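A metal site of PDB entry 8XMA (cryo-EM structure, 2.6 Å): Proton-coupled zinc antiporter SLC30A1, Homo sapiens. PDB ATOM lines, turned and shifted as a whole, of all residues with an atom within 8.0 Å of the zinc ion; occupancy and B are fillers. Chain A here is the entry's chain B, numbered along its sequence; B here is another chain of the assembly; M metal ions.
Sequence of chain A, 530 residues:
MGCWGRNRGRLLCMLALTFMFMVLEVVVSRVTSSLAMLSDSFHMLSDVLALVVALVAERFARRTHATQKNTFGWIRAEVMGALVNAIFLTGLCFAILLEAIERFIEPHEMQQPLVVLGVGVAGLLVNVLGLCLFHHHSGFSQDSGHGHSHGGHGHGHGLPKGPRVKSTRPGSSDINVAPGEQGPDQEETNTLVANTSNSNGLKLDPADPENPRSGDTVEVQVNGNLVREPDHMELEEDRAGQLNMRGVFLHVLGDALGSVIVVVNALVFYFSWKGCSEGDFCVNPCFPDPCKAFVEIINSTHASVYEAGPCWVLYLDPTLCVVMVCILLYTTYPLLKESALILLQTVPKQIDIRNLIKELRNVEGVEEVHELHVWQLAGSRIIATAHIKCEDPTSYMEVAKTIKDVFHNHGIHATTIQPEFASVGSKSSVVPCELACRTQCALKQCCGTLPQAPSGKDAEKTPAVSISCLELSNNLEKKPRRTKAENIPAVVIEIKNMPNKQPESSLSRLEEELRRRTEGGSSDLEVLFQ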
ATOM      1  N   GLU A 368      -2.961 -26.516  13.407  1.00  0.00           N
ATOM      2  CA  GLU A 368      -2.511 -27.753  14.018  1.00  0.00           C
ATOM      3  C   GLU A 368      -1.586 -27.410  15.177  1.00  0.00           C
ATOM      4  O   GLU A 368      -0.907 -26.387  15.167  1.00  0.00           O
ATOM      5  CB  GLU A 368      -1.810 -28.668  13.000  1.00  0.00           C
ATOM      6  CG  GLU A 368      -0.550 -28.098  12.368  1.00  0.00           C
ATOM      7  CD  GLU A 368       0.697 -28.341  13.203  1.00  0.00           C
ATOM      8  OE1 GLU A 368       0.661 -29.250  14.058  1.00  0.00           O
ATOM      9  OE2 GLU A 368       1.690 -27.624  13.004  1.00  0.00           O
ATOM     10  N   VAL A 369      -1.574 -28.289  16.185  1.00  0.00           N
ATOM     11  CA  VAL A 369      -0.774 -28.101  17.381  1.00  0.00           C
ATOM     12  C   VAL A 369       0.197 -29.267  17.511  1.00  0.00           C
ATOM     13  O   VAL A 369      -0.217 -30.423  17.507  1.00  0.00           O
ATOM     14  CB  VAL A 369      -1.658 -27.992  18.640  1.00  0.00           C
ATOM     15  CG1 VAL A 369      -0.786 -27.913  19.887  1.00  0.00           C
ATOM     16  CG2 VAL A 369      -2.580 -26.783  18.543  1.00  0.00           C
ATOM     17  N   HIS A 370       1.488 -28.946  17.619  1.00  0.00           N
ATOM     18  CA  HIS A 370       2.520 -29.965  17.775  1.00  0.00           C
ATOM     19  C   HIS A 370       3.528 -29.503  18.808  1.00  0.00           C
ATOM     20  O   HIS A 370       3.603 -28.318  19.149  1.00  0.00           O
ATOM     21  CB  HIS A 370       3.220 -30.259  16.435  1.00  0.00           C
ATOM     22  CG  HIS A 370       4.082 -29.143  15.955  1.00  0.00           C
ATOM     23  ND1 HIS A 370       3.580 -28.043  15.305  1.00  0.00           N
ATOM     24  CD2 HIS A 370       5.427 -28.970  16.008  1.00  0.00           C
ATOM     25  CE1 HIS A 370       4.570 -27.225  14.990  1.00  0.00           C
ATOM     26  NE2 HIS A 370       5.704 -27.763  15.406  1.00  0.00           N
ATOM     27  N   GLU A 371       4.292 -30.456  19.329  1.00  0.00           N
ATOM     28  CA  GLU A 371       5.284 -30.218  20.374  1.00  0.00           C
ATOM     29  C   GLU A 371       4.628 -29.608  21.617  1.00  0.00           C
ATOM     30  O   GLU A 371       5.001 -28.540  22.093  1.00  0.00           O
ATOM     31  CB  GLU A 371       6.422 -29.335  19.847  1.00  0.00           C
ATOM     32  CG  GLU A 371       7.676 -29.354  20.704  1.00  0.00           C
ATOM     33  CD  GLU A 371       8.499 -30.605  20.497  1.00  0.00           C
ATOM     34  OE1 GLU A 371       8.483 -31.157  19.376  1.00  0.00           O
ATOM     35  OE2 GLU A 371       9.166 -31.044  21.460  1.00  0.00           O
ATOM     36  N   LEU A 372       3.625 -30.318  22.117  1.00  0.00           N
ATOM     37  CA  LEU A 372       2.924 -29.910  23.336  1.00  0.00           C
ATOM     38  C   LEU A 372       3.587 -30.570  24.535  1.00  0.00           C
ATOM     39  O   LEU A 372       3.620 -31.796  24.640  1.00  0.00           O
ATOM     40  CB  LEU A 372       1.442 -30.301  23.275  1.00  0.00           C
ATOM     41  CG  LEU A 372       0.653 -29.946  24.534  1.00  0.00           C
ATOM     42  CD1 LEU A 372       0.257 -28.488  24.531  1.00  0.00           C
ATOM     43  CD2 LEU A 372      -0.570 -30.837  24.676  1.00  0.00           C
ATOM     44  N   ALA A 386       3.755 -25.190  23.676  1.00  0.00           N
ATOM     45  CA  ALA A 386       3.239 -25.758  22.436  1.00  0.00           C
ATOM     46  C   ALA A 386       3.657 -24.906  21.253  1.00  0.00           C
ATOM     47  O   ALA A 386       3.976 -23.719  21.386  1.00  0.00           O
ATOM     48  CB  ALA A 386       1.710 -25.879  22.484  1.00  0.00           C
ATOM     49  N   HIS A 387       3.654 -25.527  20.082  1.00  0.00           N
ATOM     50  CA  HIS A 387       3.885 -24.854  18.810  1.00  0.00           C
ATOM     51  C   HIS A 387       2.593 -24.895  17.999  1.00  0.00           C
ATOM     52  O   HIS A 387       1.913 -25.931  17.957  1.00  0.00           O
ATOM     53  CB  HIS A 387       5.016 -25.516  18.019  1.00  0.00           C
ATOM     54  CG  HIS A 387       6.343 -25.478  18.705  1.00  0.00           C
ATOM     55  ND1 HIS A 387       7.520 -25.803  18.063  1.00  0.00           N
ATOM     56  CD2 HIS A 387       6.682 -25.171  19.984  1.00  0.00           C
ATOM     57  CE1 HIS A 387       8.519 -25.691  18.914  1.00  0.00           C
ATOM     58  NE2 HIS A 387       8.041 -25.315  20.083  1.00  0.00           N
ATOM     59  N   ILE A 388       2.257 -23.784  17.355  1.00  0.00           N
ATOM     60  CA  ILE A 388       1.015 -23.690  16.596  1.00  0.00           C
ATOM     61  C   ILE A 388       1.317 -23.127  15.218  1.00  0.00           C
ATOM     62  O   ILE A 388       2.339 -22.461  15.001  1.00  0.00           O
ATOM     63  CB  ILE A 388      -0.034 -22.805  17.303  1.00  0.00           C
ATOM     64  CG1 ILE A 388       0.530 -21.419  17.563  1.00  0.00           C
ATOM     65  CG2 ILE A 388      -0.483 -23.463  18.608  1.00  0.00           C
ATOM     66  CD1 ILE A 388      -0.509 -20.409  17.994  1.00  0.00           C
ATOM     67  N   LYS A 389       0.428 -23.401  14.266  1.00  0.00           N
ATOM     68  CA  LYS A 389       0.463 -22.823  12.938  1.00  0.00           C
ATOM     69  C   LYS A 389      -0.798 -22.007  12.729  1.00  0.00           C
ATOM     70  O   LYS A 389      -1.911 -22.532  12.888  1.00  0.00           O
ATOM     71  CB  LYS A 389       0.594 -23.900  11.867  1.00  0.00           C
ATOM     72  CG  LYS A 389       1.972 -24.550  11.796  1.00  0.00           C
ATOM     73  CD  LYS A 389       2.056 -25.521  10.640  1.00  0.00           C
ATOM     74  CE  LYS A 389       3.406 -26.222  10.602  1.00  0.00           C
ATOM     75  NZ  LYS A 389       4.506 -25.285  10.228  1.00  0.00           N
ATOM     76  N   GLN A 418       4.496 -20.868  20.695  1.00  0.00           N
ATOM     77  CA  GLN A 418       5.320 -20.348  19.603  1.00  0.00           C
ATOM     78  C   GLN A 418       4.593 -20.521  18.289  1.00  0.00           C
ATOM     79  O   GLN A 418       4.394 -21.662  17.846  1.00  0.00           O
ATOM     80  CB  GLN A 418       6.667 -21.062  19.571  1.00  0.00           C
ATOM     81  CG  GLN A 418       7.442 -20.853  18.282  1.00  0.00           C
ATOM     82  CD  GLN A 418       8.481 -21.925  18.045  1.00  0.00           C
ATOM     83  OE1 GLN A 418       9.343 -22.156  18.885  1.00  0.00           O
ATOM     84  NE2 GLN A 418       8.401 -22.577  16.896  1.00  0.00           N
ATOM     85  N   PRO A 419       4.178 -19.442  17.625  1.00  0.00           N
ATOM     86  CA  PRO A 419       3.513 -19.580  16.330  1.00  0.00           C
ATOM     87  C   PRO A 419       4.509 -19.931  15.233  1.00  0.00           C
ATOM     88  O   PRO A 419       5.708 -19.645  15.325  1.00  0.00           O
ATOM     89  CB  PRO A 419       2.901 -18.195  16.084  1.00  0.00           C
ATOM     90  CG  PRO A 419       3.117 -17.420  17.351  1.00  0.00           C
ATOM     91  CD  PRO A 419       4.270 -18.043  18.046  1.00  0.00           C
ATOM     92  N   GLU A 420       3.994 -20.560  14.186  1.00  0.00           N
ATOM     93  CA  GLU A 420       4.760 -20.836  12.978  1.00  0.00           C
ATOM     94  C   GLU A 420       3.898 -20.490  11.772  1.00  0.00           C
ATOM     95  O   GLU A 420       2.713 -20.844  11.729  1.00  0.00           O
ATOM     96  CB  GLU A 420       5.204 -22.295  12.907  1.00  0.00           C
ATOM     97  CG  GLU A 420       5.961 -22.772  14.141  1.00  0.00           C
ATOM     98  CD  GLU A 420       6.213 -24.272  14.129  1.00  0.00           C
ATOM     99  OE1 GLU A 420       6.077 -24.890  13.057  1.00  0.00           O
ATOM    100  OE2 GLU A 420       6.549 -24.816  15.197  1.00  0.00           O
ATOM    101  N   PRO A 432       7.382 -31.086   9.578  1.00  0.00           N
ATOM    102  CA  PRO A 432       6.508 -31.050  10.757  1.00  0.00           C
ATOM    103  C   PRO A 432       6.630 -29.753  11.548  1.00  0.00           C
ATOM    104  O   PRO A 432       5.625 -29.255  12.068  1.00  0.00           O
ATOM    105  CB  PRO A 432       6.951 -32.274  11.571  1.00  0.00           C
ATOM    106  CG  PRO A 432       8.355 -32.523  11.123  1.00  0.00           C
ATOM    107  CD  PRO A 432       8.394 -32.157   9.675  1.00  0.00           C
ATOM    108  N   CYS A 433       7.841 -29.217  11.653  1.00  0.00           N
ATOM    109  CA  CYS A 433       8.079 -27.993  12.413  1.00  0.00           C
ATOM    110  C   CYS A 433       9.048 -27.093  11.661  1.00  0.00           C
ATOM    111  O   CYS A 433      10.204 -27.472  11.447  1.00  0.00           O
ATOM    112  CB  CYS A 433       8.620 -28.320  13.806  1.00  0.00           C
ATOM    113  SG  CYS A 433       8.897 -26.890  14.885  1.00  0.00           S
ATOM    114  N   GLU A 434       8.591 -25.915  11.263  1.00  0.00           N
ATOM    115  CA  GLU A 434       9.447 -25.001  10.491  1.00  0.00           C
ATOM    116  C   GLU A 434      10.665 -24.520  11.265  1.00  0.00           C
ATOM    117  O   GLU A 434      11.765 -24.442  10.701  1.00  0.00           O
ATOM    118  CB  GLU A 434       8.631 -23.802  10.018  1.00  0.00           C
ATOM    119  CG  GLU A 434       7.593 -24.152   8.981  1.00  0.00           C
ATOM    120  CD  GLU A 434       6.466 -23.142   8.949  1.00  0.00           C
ATOM    121  OE1 GLU A 434       6.450 -22.251   9.823  1.00  0.00           O
ATOM    122  OE2 GLU A 434       5.594 -23.252   8.063  1.00  0.00           O
ATOM    123  N   LEU A 435      10.491 -24.203  12.541  1.00  0.00           N
ATOM    124  CA  LEU A 435      11.628 -23.779  13.348  1.00  0.00           C
ATOM    125  C   LEU A 435      12.357 -24.997  13.887  1.00  0.00           C
ATOM    126  O   LEU A 435      12.200 -25.364  15.049  1.00  0.00           O
ATOM    127  CB  LEU A 435      11.173 -22.892  14.506  1.00  0.00           C
ATOM    128  CG  LEU A 435      11.128 -21.389  14.221  1.00  0.00           C
ATOM    129  CD1 LEU A 435      10.934 -20.627  15.516  1.00  0.00           C
ATOM    130  CD2 LEU A 435      12.417 -20.963  13.552  1.00  0.00           C
ATOM    131  N   ALA A 436      13.178 -25.619  13.036  1.00  0.00           N
ATOM    132  CA  ALA A 436      13.880 -26.825  13.459  1.00  0.00           C
ATOM    133  C   ALA A 436      15.377 -26.583  13.387  1.00  0.00           C
ATOM    134  O   ALA A 436      15.864 -25.720  12.645  1.00  0.00           O
ATOM    135  CB  ALA A 436      13.498 -28.026  12.591  1.00  0.00           C
ATOM    136  N   LYS B 404      16.507 -18.719  16.752  1.00  0.00           N
ATOM    137  CA  LYS B 404      16.826 -20.147  16.699  1.00  0.00           C
ATOM    138  C   LYS B 404      18.307 -20.366  16.459  1.00  0.00           C
ATOM    139  O   LYS B 404      18.928 -21.234  17.067  1.00  0.00           O
ATOM    140  CB  LYS B 404      15.993 -20.836  15.629  1.00  0.00           C
ATOM    141  CG  LYS B 404      16.224 -22.336  15.528  1.00  0.00           C
ATOM    142  CD  LYS B 404      15.815 -23.075  16.784  1.00  0.00           C
ATOM    143  CE  LYS B 404      14.310 -23.068  16.951  1.00  0.00           C
ATOM    144  NZ  LYS B 404      13.884 -23.845  18.143  1.00  0.00           N
ATOM    145  N   THR B 415      13.865 -25.373  21.569  1.00  0.00           N
ATOM    146  CA  THR B 415      13.476 -24.072  22.078  1.00  0.00           C
ATOM    147  C   THR B 415      11.998 -23.798  21.788  1.00  0.00           C
ATOM    148  O   THR B 415      11.327 -24.543  21.074  1.00  0.00           O
ATOM    149  CB  THR B 415      14.339 -22.966  21.462  1.00  0.00           C
ATOM    150  OG1 THR B 415      13.917 -22.720  20.115  1.00  0.00           O
ATOM    151  CG2 THR B 415      15.792 -23.380  21.451  1.00  0.00           C
ATOM    152  N   THR B 416      11.517 -22.710  22.381  1.00  0.00           N
ATOM    153  CA  THR B 416      10.156 -22.237  22.137  1.00  0.00           C
ATOM    154  C   THR B 416      10.121 -20.746  22.440  1.00  0.00           C
ATOM    155  O   THR B 416      10.293 -20.349  23.595  1.00  0.00           O
ATOM    156  CB  THR B 416       9.146 -22.986  22.998  1.00  0.00           C
ATOM    157  OG1 THR B 416       9.143 -24.374  22.646  1.00  0.00           O
ATOM    158  CG2 THR B 416       7.750 -22.417  22.783  1.00  0.00           C
HETATM  159 ZN    ZN M   1       7.011 -26.455  16.218  1.00  0.00          ZN
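The zinc ion is bound by the side-chain carboxylate of Glu 420 (2.0 Å), a ring nitrogen (NE2) of His 370 (2.0 Å), a ring nitrogen (ND1) of His 387 (2.0 Å) and the side-chain sulfur of Cys 433 (2.4 Å).
The backbone NH of Glu 434 sits at hydrogen-bond distance from the side-chain carboxylate of Glu 420 (3.3 Å).
The backbone NH (N) of Glu 420 is in hydrogen-bond range of the backbone carbonyl oxygen (O) of Ile 388 (2.6 Å).
A ring nitrogen (ND1) of His 370 is in hydrogen-bond range of the side-chain carboxylate (OE2) of Glu 368, at 3.0 Å.
OG1 of Thr 416 of chain B is in hydrogen-bond range of NE2 of His 387, 2.9 Å away.
The side-chain sulfur of Cys 433 sits close to the backbone carbonyl oxygen of Leu 435.
The side-chain amide nitrogen (NE2) of Gln 418 lies close to the side-chain carboxylate (OE2) of Glu 420 (3.4 Å).
The side-chain amino group (NZ) of Lys 389 lies within salt-bridge range of the side-chain carboxylate (OE1) of Glu 420 (3.3 Å).
The nearest printed residue that does not touch the zinc ion is Gln 418 (4.2 Å).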
